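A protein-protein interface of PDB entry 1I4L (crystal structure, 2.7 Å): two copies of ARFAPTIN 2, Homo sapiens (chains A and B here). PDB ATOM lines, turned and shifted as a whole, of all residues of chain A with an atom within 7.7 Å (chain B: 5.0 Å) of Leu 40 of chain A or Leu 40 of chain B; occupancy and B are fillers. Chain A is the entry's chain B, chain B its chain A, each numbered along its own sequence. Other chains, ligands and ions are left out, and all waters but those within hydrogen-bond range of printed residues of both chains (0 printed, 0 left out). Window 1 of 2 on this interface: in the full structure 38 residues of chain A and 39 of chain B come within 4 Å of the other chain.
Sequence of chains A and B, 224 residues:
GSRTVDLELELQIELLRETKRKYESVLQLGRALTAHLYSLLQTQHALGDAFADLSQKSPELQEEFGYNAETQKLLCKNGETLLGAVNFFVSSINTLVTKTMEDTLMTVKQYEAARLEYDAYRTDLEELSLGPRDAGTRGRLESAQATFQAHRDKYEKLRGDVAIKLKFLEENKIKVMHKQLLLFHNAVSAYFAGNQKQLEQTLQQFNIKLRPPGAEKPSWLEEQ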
ATOM      1  N   ALA A  32      13.294 -22.866  11.557  1.00  0.00           N
ATOM      2  CA  ALA A  32      13.007 -23.452  12.851  1.00  0.00           C
ATOM      3  C   ALA A  32      11.493 -23.553  12.958  1.00  0.00           C
ATOM      4  O   ALA A  32      10.945 -24.628  13.201  1.00  0.00           O
ATOM      5  CB  ALA A  32      13.544 -22.566  13.956  1.00  0.00           C
ATOM      6  N   LEU A  33      10.827 -22.417  12.760  1.00  0.00           N
ATOM      7  CA  LEU A  33       9.377 -22.350  12.835  1.00  0.00           C
ATOM      8  C   LEU A  33       8.787 -23.401  11.929  1.00  0.00           C
ATOM      9  O   LEU A  33       7.801 -24.047  12.269  1.00  0.00           O
ATOM     10  CB  LEU A  33       8.893 -20.972  12.406  1.00  0.00           C
ATOM     11  CG  LEU A  33       7.387 -20.749  12.516  1.00  0.00           C
ATOM     12  CD1 LEU A  33       6.919 -20.968  13.941  1.00  0.00           C
ATOM     13  CD2 LEU A  33       7.073 -19.345  12.079  1.00  0.00           C
ATOM     14  N   THR A  34       9.407 -23.568  10.769  1.00  0.00           N
ATOM     15  CA  THR A  34       8.956 -24.553   9.801  1.00  0.00           C
ATOM     16  C   THR A  34       9.082 -25.915  10.472  1.00  0.00           C
ATOM     17  O   THR A  34       8.116 -26.666  10.589  1.00  0.00           O
ATOM     18  CB  THR A  34       9.853 -24.553   8.553  1.00  0.00           C
ATOM     19  OG1 THR A  34      10.289 -23.216   8.267  1.00  0.00           O
ATOM     20  CG2 THR A  34       9.095 -25.097   7.366  1.00  0.00           C
ATOM     21  N   ALA A  35      10.300 -26.213  10.916  1.00  0.00           N
ATOM     22  CA  ALA A  35      10.630 -27.469  11.585  1.00  0.00           C
ATOM     23  C   ALA A  35       9.632 -27.829  12.672  1.00  0.00           C
ATOM     24  O   ALA A  35       8.875 -28.787  12.551  1.00  0.00           O
ATOM     25  CB  ALA A  35      12.019 -27.371  12.188  1.00  0.00           C
ATOM     26  N   HIS A  36       9.639 -27.052  13.743  1.00  0.00           N
ATOM     27  CA  HIS A  36       8.736 -27.311  14.839  1.00  0.00           C
ATOM     28  C   HIS A  36       7.284 -27.435  14.391  1.00  0.00           C
ATOM     29  O   HIS A  36       6.543 -28.269  14.904  1.00  0.00           O
ATOM     30  CB  HIS A  36       8.880 -26.223  15.894  1.00  0.00           C
ATOM     31  CG  HIS A  36      10.292 -25.997  16.323  1.00  0.00           C
ATOM     32  ND1 HIS A  36      11.299 -26.904  16.070  1.00  0.00           N
ATOM     33  CD2 HIS A  36      10.868 -24.974  16.999  1.00  0.00           C
ATOM     34  CE1 HIS A  36      12.434 -26.448  16.568  1.00  0.00           C
ATOM     35  NE2 HIS A  36      12.199 -25.279  17.138  1.00  0.00           N
ATOM     36  N   LEU A  37       6.878 -26.625  13.419  1.00  0.00           N
ATOM     37  CA  LEU A  37       5.497 -26.665  12.943  1.00  0.00           C
ATOM     38  C   LEU A  37       5.185 -27.985  12.262  1.00  0.00           C
ATOM     39  O   LEU A  37       4.124 -28.566  12.461  1.00  0.00           O
ATOM     40  CB  LEU A  37       5.242 -25.520  11.965  1.00  0.00           C
ATOM     41  CG  LEU A  37       3.790 -25.078  11.853  1.00  0.00           C
ATOM     42  CD1 LEU A  37       3.361 -24.399  13.148  1.00  0.00           C
ATOM     43  CD2 LEU A  37       3.654 -24.121  10.685  1.00  0.00           C
ATOM     44  N   TYR A  38       6.123 -28.446  11.453  1.00  0.00           N
ATOM     45  CA  TYR A  38       5.969 -29.698  10.723  1.00  0.00           C
ATOM     46  C   TYR A  38       5.769 -30.848  11.708  1.00  0.00           C
ATOM     47  O   TYR A  38       4.821 -31.620  11.594  1.00  0.00           O
ATOM     48  CB  TYR A  38       7.210 -29.949   9.868  1.00  0.00           C
ATOM     49  CG  TYR A  38       7.158 -31.234   9.090  1.00  0.00           C
ATOM     50  CD1 TYR A  38       6.232 -31.407   8.062  1.00  0.00           C
ATOM     51  CD2 TYR A  38       8.015 -32.296   9.394  1.00  0.00           C
ATOM     52  CE1 TYR A  38       6.157 -32.605   7.357  1.00  0.00           C
ATOM     53  CE2 TYR A  38       7.945 -33.501   8.694  1.00  0.00           C
ATOM     54  CZ  TYR A  38       7.011 -33.644   7.680  1.00  0.00           C
ATOM     55  OH  TYR A  38       6.909 -34.831   6.995  1.00  0.00           O
ATOM     56  N   SER A  39       6.674 -30.948  12.677  1.00  0.00           N
ATOM     57  CA  SER A  39       6.607 -31.979  13.696  1.00  0.00           C
ATOM     58  C   SER A  39       5.245 -31.955  14.364  1.00  0.00           C
ATOM     59  O   SER A  39       4.527 -32.942  14.375  1.00  0.00           O
ATOM     60  CB  SER A  39       7.681 -31.739  14.755  1.00  0.00           C
ATOM     61  OG  SER A  39       8.974 -31.731  14.183  1.00  0.00           O
ATOM     62  N   LEU A  40       4.890 -30.810  14.922  1.00  0.00           N
ATOM     63  CA  LEU A  40       3.625 -30.658  15.605  1.00  0.00           C
ATOM     64  C   LEU A  40       2.462 -31.185  14.783  1.00  0.00           C
ATOM     65  O   LEU A  40       1.499 -31.698  15.333  1.00  0.00           O
ATOM     66  CB  LEU A  40       3.392 -29.194  15.940  1.00  0.00           C
ATOM     67  CG  LEU A  40       2.187 -28.901  16.830  1.00  0.00           C
ATOM     68  CD1 LEU A  40       2.517 -29.265  18.268  1.00  0.00           C
ATOM     69  CD2 LEU A  40       1.839 -27.417  16.739  1.00  0.00           C
ATOM     70  N   LEU A  41       2.543 -31.068  13.466  1.00  0.00           N
ATOM     71  CA  LEU A  41       1.450 -31.542  12.634  1.00  0.00           C
ATOM     72  C   LEU A  41       1.428 -33.051  12.591  1.00  0.00           C
ATOM     73  O   LEU A  41       0.357 -33.661  12.646  1.00  0.00           O
ATOM     74  CB  LEU A  41       1.556 -30.963  11.216  1.00  0.00           C
ATOM     75  CG  LEU A  41       1.147 -29.486  11.097  1.00  0.00           C
ATOM     76  CD1 LEU A  41       1.288 -29.015   9.668  1.00  0.00           C
ATOM     77  CD2 LEU A  41      -0.288 -29.321  11.567  1.00  0.00           C
ATOM     78  N   GLN A  42       2.611 -33.649  12.485  1.00  0.00           N
ATOM     79  CA  GLN A  42       2.756 -35.107  12.452  1.00  0.00           C
ATOM     80  C   GLN A  42       2.109 -35.698  13.699  1.00  0.00           C
ATOM     81  O   GLN A  42       1.396 -36.694  13.644  1.00  0.00           O
ATOM     82  CB  GLN A  42       4.235 -35.486  12.456  1.00  0.00           C
ATOM     83  CG  GLN A  42       5.035 -34.928  11.304  1.00  0.00           C
ATOM     84  CD  GLN A  42       4.579 -35.485   9.975  1.00  0.00           C
ATOM     85  OE1 GLN A  42       3.421 -35.316   9.578  1.00  0.00           O
ATOM     86  NE2 GLN A  42       5.490 -36.161   9.275  1.00  0.00           N
ATOM     87  N   THR A  43       2.377 -35.050  14.823  1.00  0.00           N
ATOM     88  CA  THR A  43       1.870 -35.460  16.112  1.00  0.00           C
ATOM     89  C   THR A  43       0.355 -35.334  16.198  1.00  0.00           C
ATOM     90  O   THR A  43      -0.334 -36.236  16.688  1.00  0.00           O
ATOM     91  CB  THR A  43       2.520 -34.610  17.203  1.00  0.00           C
ATOM     92  OG1 THR A  43       3.947 -34.708  17.084  1.00  0.00           O
ATOM     93  CG2 THR A  43       2.084 -35.061  18.581  1.00  0.00           C
ATOM     94  N   GLN A  44      -0.172 -34.216  15.724  1.00  0.00           N
ATOM     95  CA  GLN A  44      -1.605 -34.012  15.766  1.00  0.00           C
ATOM     96  C   GLN A  44      -2.314 -34.988  14.825  1.00  0.00           C
ATOM     97  O   GLN A  44      -3.431 -35.426  15.100  1.00  0.00           O
ATOM     98  CB  GLN A  44      -1.929 -32.567  15.407  1.00  0.00           C
ATOM     99  CG  GLN A  44      -1.262 -31.569  16.330  1.00  0.00           C
ATOM    100  CD  GLN A  44      -1.558 -30.132  15.960  1.00  0.00           C
ATOM    101  OE1 GLN A  44      -2.686 -29.665  16.080  1.00  0.00           O
ATOM    102  NE2 GLN A  44      -0.543 -29.427  15.501  1.00  0.00           N
ATOM    103  N   HIS A  45      -1.662 -35.335  13.721  1.00  0.00           N
ATOM    104  CA  HIS A  45      -2.245 -36.278  12.768  1.00  0.00           C
ATOM    105  C   HIS A  45      -2.354 -37.664  13.432  1.00  0.00           C
ATOM    106  O   HIS A  45      -3.411 -38.304  13.428  1.00  0.00           O
ATOM    107  CB  HIS A  45      -1.369 -36.356  11.516  1.00  0.00           C
ATOM    108  CG  HIS A  45      -1.878 -37.308  10.485  1.00  0.00           C
ATOM    109  ND1 HIS A  45      -3.175 -37.273  10.017  1.00  0.00           N
ATOM    110  CD2 HIS A  45      -1.270 -38.327   9.833  1.00  0.00           C
ATOM    111  CE1 HIS A  45      -3.345 -38.233   9.122  1.00  0.00           C
ATOM    112  NE2 HIS A  45      -2.204 -38.886   8.993  1.00  0.00           N
ATOM    113  N   ALA A  46      -1.246 -38.101  14.018  1.00  0.00           N
ATOM    114  CA  ALA A  46      -1.174 -39.375  14.709  1.00  0.00           C
ATOM    115  C   ALA A  46      -2.106 -39.399  15.912  1.00  0.00           C
ATOM    116  O   ALA A  46      -2.692 -40.433  16.242  1.00  0.00           O
ATOM    117  CB  ALA A  46       0.244 -39.616  15.168  1.00  0.00           C
ATOM    118  N   LEU A  47      -2.234 -38.255  16.572  1.00  0.00           N
ATOM    119  CA  LEU A  47      -3.064 -38.161  17.759  1.00  0.00           C
ATOM    120  C   LEU A  47      -4.547 -38.217  17.415  1.00  0.00           C
ATOM    121  O   LEU A  47      -5.355 -38.755  18.176  1.00  0.00           O
ATOM    122  CB  LEU A  47      -2.711 -36.882  18.511  1.00  0.00           C
ATOM    123  CG  LEU A  47      -3.179 -36.727  19.954  1.00  0.00           C
ATOM    124  CD1 LEU A  47      -2.967 -38.006  20.739  1.00  0.00           C
ATOM    125  CD2 LEU A  47      -2.413 -35.572  20.573  1.00  0.00           C
ATOM    126  N   GLN A  72      -8.361 -32.374  16.534  1.00  0.00           N
ATOM    127  CA  GLN A  72      -6.992 -32.576  16.113  1.00  0.00           C
ATOM    128  C   GLN A  72      -6.915 -32.715  14.591  1.00  0.00           C
ATOM    129  O   GLN A  72      -5.960 -32.273  13.960  1.00  0.00           O
ATOM    130  CB  GLN A  72      -6.436 -33.813  16.817  1.00  0.00           C
ATOM    131  CG  GLN A  72      -4.968 -33.747  17.206  1.00  0.00           C
ATOM    132  CD  GLN A  72      -4.648 -32.696  18.265  1.00  0.00           C
ATOM    133  OE1 GLN A  72      -5.441 -32.424  19.175  1.00  0.00           O
ATOM    134  NE2 GLN A  72      -3.465 -32.124  18.163  1.00  0.00           N
ATOM    135  N   LEU A  75      -7.356 -29.224  13.043  1.00  0.00           N
ATOM    136  CA  LEU A  75      -6.131 -28.496  13.334  1.00  0.00           C
ATOM    137  C   LEU A  75      -4.999 -28.879  12.389  1.00  0.00           C
ATOM    138  O   LEU A  75      -4.224 -28.037  11.942  1.00  0.00           O
ATOM    139  CB  LEU A  75      -5.704 -28.783  14.767  1.00  0.00           C
ATOM    140  CG  LEU A  75      -5.863 -27.685  15.813  1.00  0.00           C
ATOM    141  CD1 LEU A  75      -7.226 -27.007  15.717  1.00  0.00           C
ATOM    142  CD2 LEU A  75      -5.659 -28.337  17.173  1.00  0.00           C
ATOM    143  N   CYS A  76      -4.912 -30.166  12.096  1.00  0.00           N
ATOM    144  CA  CYS A  76      -3.874 -30.699  11.224  1.00  0.00           C
ATOM    145  C   CYS A  76      -4.094 -30.165   9.803  1.00  0.00           C
ATOM    146  O   CYS A  76      -3.165 -29.692   9.144  1.00  0.00           O
ATOM    147  CB  CYS A  76      -3.925 -32.237  11.272  1.00  0.00           C
ATOM    148  SG  CYS A  76      -2.566 -33.117  10.451  1.00  0.00           S
ATOM    149  N   LEU A  82      -1.108 -23.215   6.774  1.00  0.00           N
ATOM    150  CA  LEU A  82      -0.180 -22.356   7.496  1.00  0.00           C
ATOM    151  C   LEU A  82       1.264 -22.701   7.163  1.00  0.00           C
ATOM    152  O   LEU A  82       2.099 -21.822   6.930  1.00  0.00           O
ATOM    153  CB  LEU A  82      -0.390 -22.488   9.004  1.00  0.00           C
ATOM    154  CG  LEU A  82       0.720 -21.835   9.826  1.00  0.00           C
ATOM    155  CD1 LEU A  82       0.884 -20.375   9.414  1.00  0.00           C
ATOM    156  CD2 LEU A  82       0.394 -21.937  11.295  1.00  0.00           C
ATOM    157  N   TYR A 191      -5.062 -18.720  10.232  1.00  0.00           N
ATOM    158  CA  TYR A 191      -4.919 -19.982  10.924  1.00  0.00           C
ATOM    159  C   TYR A 191      -5.931 -20.055  12.051  1.00  0.00           C
ATOM    160  O   TYR A 191      -6.833 -20.884  12.033  1.00  0.00           O
ATOM    161  CB  TYR A 191      -3.503 -20.106  11.485  1.00  0.00           C
ATOM    162  CG  TYR A 191      -3.224 -21.416  12.168  1.00  0.00           C
ATOM    163  CD1 TYR A 191      -3.227 -22.614  11.450  1.00  0.00           C
ATOM    164  CD2 TYR A 191      -2.980 -21.470  13.536  1.00  0.00           C
ATOM    165  CE1 TYR A 191      -2.997 -23.833  12.080  1.00  0.00           C
ATOM    166  CE2 TYR A 191      -2.746 -22.687  14.173  1.00  0.00           C
ATOM    167  CZ  TYR A 191      -2.760 -23.858  13.438  1.00  0.00           C
ATOM    168  OH  TYR A 191      -2.552 -25.056  14.070  1.00  0.00           O
ATOM    169  N   LEU B  33       4.128 -33.973  21.710  1.00  0.00           N
ATOM    170  CA  LEU B  33       3.343 -32.763  21.602  1.00  0.00           C
ATOM    171  C   LEU B  33       3.909 -31.700  22.519  1.00  0.00           C
ATOM    172  O   LEU B  33       3.946 -30.525  22.176  1.00  0.00           O
ATOM    173  CB  LEU B  33       1.896 -33.047  21.978  1.00  0.00           C
ATOM    174  CG  LEU B  33       0.951 -31.866  21.833  1.00  0.00           C
ATOM    175  CD1 LEU B  33       0.967 -31.410  20.391  1.00  0.00           C
ATOM    176  CD2 LEU B  33      -0.454 -32.260  22.259  1.00  0.00           C
ATOM    177  N   ALA B  35       7.066 -31.470  23.543  1.00  0.00           N
ATOM    178  CA  ALA B  35       8.389 -31.078  23.077  1.00  0.00           C
ATOM    179  C   ALA B  35       8.258 -30.001  22.022  1.00  0.00           C
ATOM    180  O   ALA B  35       8.699 -28.855  22.197  1.00  0.00           O
ATOM    181  CB  ALA B  35       9.103 -32.283  22.486  1.00  0.00           C
ATOM    182  N   HIS B  36       7.647 -30.414  20.919  1.00  0.00           N
ATOM    183  CA  HIS B  36       7.396 -29.574  19.769  1.00  0.00           C
ATOM    184  C   HIS B  36       6.736 -28.256  20.140  1.00  0.00           C
ATOM    185  O   HIS B  36       7.078 -27.211  19.607  1.00  0.00           O
ATOM    186  CB  HIS B  36       6.532 -30.359  18.813  1.00  0.00           C
ATOM    187  CG  HIS B  36       7.156 -31.647  18.398  1.00  0.00           C
ATOM    188  ND1 HIS B  36       6.420 -32.735  17.988  1.00  0.00           N
ATOM    189  CD2 HIS B  36       8.456 -32.016  18.319  1.00  0.00           C
ATOM    190  CE1 HIS B  36       7.240 -33.722  17.671  1.00  0.00           C
ATOM    191  NE2 HIS B  36       8.481 -33.311  17.863  1.00  0.00           N
ATOM    192  N   LEU B  37       5.805 -28.311  21.075  1.00  0.00           N
ATOM    193  CA  LEU B  37       5.109 -27.118  21.496  1.00  0.00           C
ATOM    194  C   LEU B  37       6.038 -26.173  22.247  1.00  0.00           C
ATOM    195  O   LEU B  37       5.889 -24.954  22.174  1.00  0.00           O
ATOM    196  CB  LEU B  37       3.930 -27.509  22.370  1.00  0.00           C
ATOM    197  CG  LEU B  37       2.931 -26.407  22.629  1.00  0.00           C
ATOM    198  CD1 LEU B  37       2.458 -25.835  21.301  1.00  0.00           C
ATOM    199  CD2 LEU B  37       1.781 -26.968  23.420  1.00  0.00           C
ATOM    200  N   TYR B  38       6.993 -26.741  22.975  1.00  0.00           N
ATOM    201  CA  TYR B  38       7.961 -25.950  23.744  1.00  0.00           C
ATOM    202  C   TYR B  38       8.960 -25.360  22.750  1.00  0.00           C
ATOM    203  O   TYR B  38       9.465 -24.258  22.950  1.00  0.00           O
ATOM    204  CB  TYR B  38       8.667 -26.847  24.780  1.00  0.00           C
ATOM    205  CG  TYR B  38       9.850 -26.236  25.517  1.00  0.00           C
ATOM    206  CD1 TYR B  38       9.671 -25.224  26.463  1.00  0.00           C
ATOM    207  CD2 TYR B  38      11.147 -26.671  25.259  1.00  0.00           C
ATOM    208  CE1 TYR B  38      10.757 -24.662  27.131  1.00  0.00           C
ATOM    209  CE2 TYR B  38      12.236 -26.121  25.914  1.00  0.00           C
ATOM    210  CZ  TYR B  38      12.040 -25.118  26.849  1.00  0.00           C
ATOM    211  OH  TYR B  38      13.132 -24.567  27.494  1.00  0.00           O
ATOM    212  N   SER B  39       9.228 -26.098  21.675  1.00  0.00           N
ATOM    213  CA  SER B  39      10.141 -25.633  20.639  1.00  0.00           C
ATOM    214  C   SER B  39       9.479 -24.524  19.822  1.00  0.00           C
ATOM    215  O   SER B  39      10.114 -23.527  19.472  1.00  0.00           O
ATOM    216  CB  SER B  39      10.517 -26.777  19.703  1.00  0.00           C
ATOM    217  OG  SER B  39      11.614 -27.502  20.206  1.00  0.00           O
ATOM    218  N   LEU B  40       8.200 -24.713  19.512  1.00  0.00           N
ATOM    219  CA  LEU B  40       7.456 -23.739  18.737  1.00  0.00           C
ATOM    220  C   LEU B  40       7.396 -22.458  19.552  1.00  0.00           C
ATOM    221  O   LEU B  40       7.729 -21.377  19.073  1.00  0.00           O
ATOM    222  CB  LEU B  40       6.046 -24.258  18.475  1.00  0.00           C
ATOM    223  CG  LEU B  40       5.255 -23.533  17.397  1.00  0.00           C
ATOM    224  CD1 LEU B  40       5.922 -23.764  16.060  1.00  0.00           C
ATOM    225  CD2 LEU B  40       3.839 -24.050  17.369  1.00  0.00           C
ATOM    226  N   LEU B  41       6.974 -22.604  20.798  1.00  0.00           N
ATOM    227  CA  LEU B  41       6.863 -21.491  21.720  1.00  0.00           C
ATOM    228  C   LEU B  41       8.096 -20.584  21.656  1.00  0.00           C
ATOM    229  O   LEU B  41       8.029 -19.465  21.150  1.00  0.00           O
ATOM    230  CB  LEU B  41       6.699 -22.034  23.133  1.00  0.00           C
ATOM    231  CG  LEU B  41       5.625 -21.386  24.002  1.00  0.00           C
ATOM    232  CD1 LEU B  41       4.280 -21.461  23.274  1.00  0.00           C
ATOM    233  CD2 LEU B  41       5.553 -22.099  25.361  1.00  0.00           C
ATOM    234  N   GLN B  42       9.219 -21.076  22.168  1.00  0.00           N
ATOM    235  CA  GLN B  42      10.458 -20.315  22.187  1.00  0.00           C
ATOM    236  C   GLN B  42      10.704 -19.507  20.923  1.00  0.00           C
ATOM    237  O   GLN B  42      10.988 -18.303  20.997  1.00  0.00           O
ATOM    238  CB  GLN B  42      11.635 -21.251  22.441  1.00  0.00           C
ATOM    239  CG  GLN B  42      11.789 -21.647  23.897  1.00  0.00           C
ATOM    240  CD  GLN B  42      12.783 -22.767  24.077  1.00  0.00           C
ATOM    241  OE1 GLN B  42      12.547 -23.893  23.643  1.00  0.00           O
ATOM    242  NE2 GLN B  42      13.909 -22.464  24.710  1.00  0.00           N
ATOM    243  N   THR B  43      10.610 -20.167  19.771  1.00  0.00           N
ATOM    244  CA  THR B  43      10.808 -19.501  18.483  1.00  0.00           C
ATOM    245  C   THR B  43       9.951 -18.235  18.425  1.00  0.00           C
ATOM    246  O   THR B  43      10.440 -17.128  18.198  1.00  0.00           O
ATOM    247  CB  THR B  43      10.390 -20.409  17.315  1.00  0.00           C
ATOM    248  OG1 THR B  43      11.214 -21.576  17.295  1.00  0.00           O
ATOM    249  CG2 THR B  43      10.525 -19.672  15.999  1.00  0.00           C
ATOM    250  N   GLN B  44       8.662 -18.413  18.645  1.00  0.00           N
ATOM    251  CA  GLN B  44       7.747 -17.295  18.620  1.00  0.00           C
ATOM    252  C   GLN B  44       8.219 -16.148  19.520  1.00  0.00           C
ATOM    253  O   GLN B  44       7.863 -14.988  19.293  1.00  0.00           O
ATOM    254  CB  GLN B  44       6.361 -17.785  19.012  1.00  0.00           C
ATOM    255  CG  GLN B  44       5.922 -18.938  18.126  1.00  0.00           C
ATOM    256  CD  GLN B  44       4.562 -19.451  18.485  1.00  0.00           C
ATOM    257  OE1 GLN B  44       4.300 -19.787  19.642  1.00  0.00           O
ATOM    258  NE2 GLN B  44       3.680 -19.518  17.497  1.00  0.00           N
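The side-chain hydroxyl of Thr 43 of chain A is in hydrogen-bond range of a ring nitrogen (ND1) of His 36 of chain B (3.3 Å).
O of Ala 35 of chain A sits at hydrogen-bond distance from OG of Ser 39 of chain A, 3.4 Å away. O of Leu 40 of chain A lies close to NE2 of Gln 44 of chain A (3.1 Å). OG1 of Thr 43 of chain A lies within hydrogen-bond range of O of Ser 39 of chain A. The backbone carbonyl oxygen (O) of Ser 39 of chain B lies within hydrogen-bond range of the side-chain hydroxyl (OG1) of Thr 43 of chain B, at 3.1 Å.
Hydrophobic or aromatic side chains of chain B that line the printed part of chain A: Leu 33, His 36 and Leu 40. Among the printed residues, 11 pairs touch across the chains. Among the printed residues, no Asp or Glu carboxylate lies within 4 Å of a Lys or Arg side-chain nitrogen of the other chain.
Among the printed residues, merely in contact across the chains: His 36 of chain A with Ser 39 of chain B, Leu 40 of chain A with Leu 33 of chain B, His 36 of chain A with Thr 43 of chain B, Ser 39 of chain A with His 36 of chain B, Leu 33 of chain A with Leu 40 of chain B, His 36 of chain A with Leu 40 of chain B, Thr 43 of chain A with Leu 33 of chain B, Leu 37 of chain A with Leu 40 of chain B, Leu 40 of chain A with His 36 of chain B and Leu 40 of chain A with Leu 40 of chain B.
His 36 of chain A touches Ser 39 of chain B, and with the chains exchanged Ser 39 of chain A touches His 36 of chain B. His 36 of chain A touches Thr 43 of chain B, and with the chains exchanged Thr 43 of chain A touches His 36 of chain B. Leu 37 of chain A touches Leu 40 of chain B, but with the chains exchanged Leu 40 of chain A does not touch Leu 37 of chain B (4.4 Å). Leu 40 of chain B touches its own counterpart, Leu 40 of chain A. Positions printed for both chains: 33, 35, 36, 37, 38, 39, 40, 41, 42, 43 and 44. Of the 11 pairs that touch across the chains among the printed residues, 9 have their exchanged pair printed and touching as well.
Of the printed residues of chain B, His 36 of chain A touches Ser 39, Leu 40 and Thr 43. Of the printed residues of chain B, Leu 37 of chain A touches Leu 40 (3.9 Å). Printed residues of chain B within 4 Å of Ser 39 of chain A: His 36. Of chain B, only Leu 33 (3.4 Å), His 36 (3.9 Å) and Leu 40 (3.97 Å) come within 4 Å of Leu 40 of chain A. Of the printed residues of chain B, Thr 43 of chain A touches Leu 33 (3.9 Å) and His 36 (3.3 Å). Gln 72 of chain A touches none of the printed residues of chain B. Leu 40 of chain B touches just these residues of chain A: Leu 33 (3.6 Å), His 36 (3.7 Å), Leu 37 (3.9 Å) and Leu 40 (3.97 Å). The nearest residue of chain B that does not touch Leu 40 of chain A is Leu 37 of chain B (4.4 Å). The nearest printed residue of chain B that does not touch His 36 of chain A is His 36 of chain B (4.2 Å).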
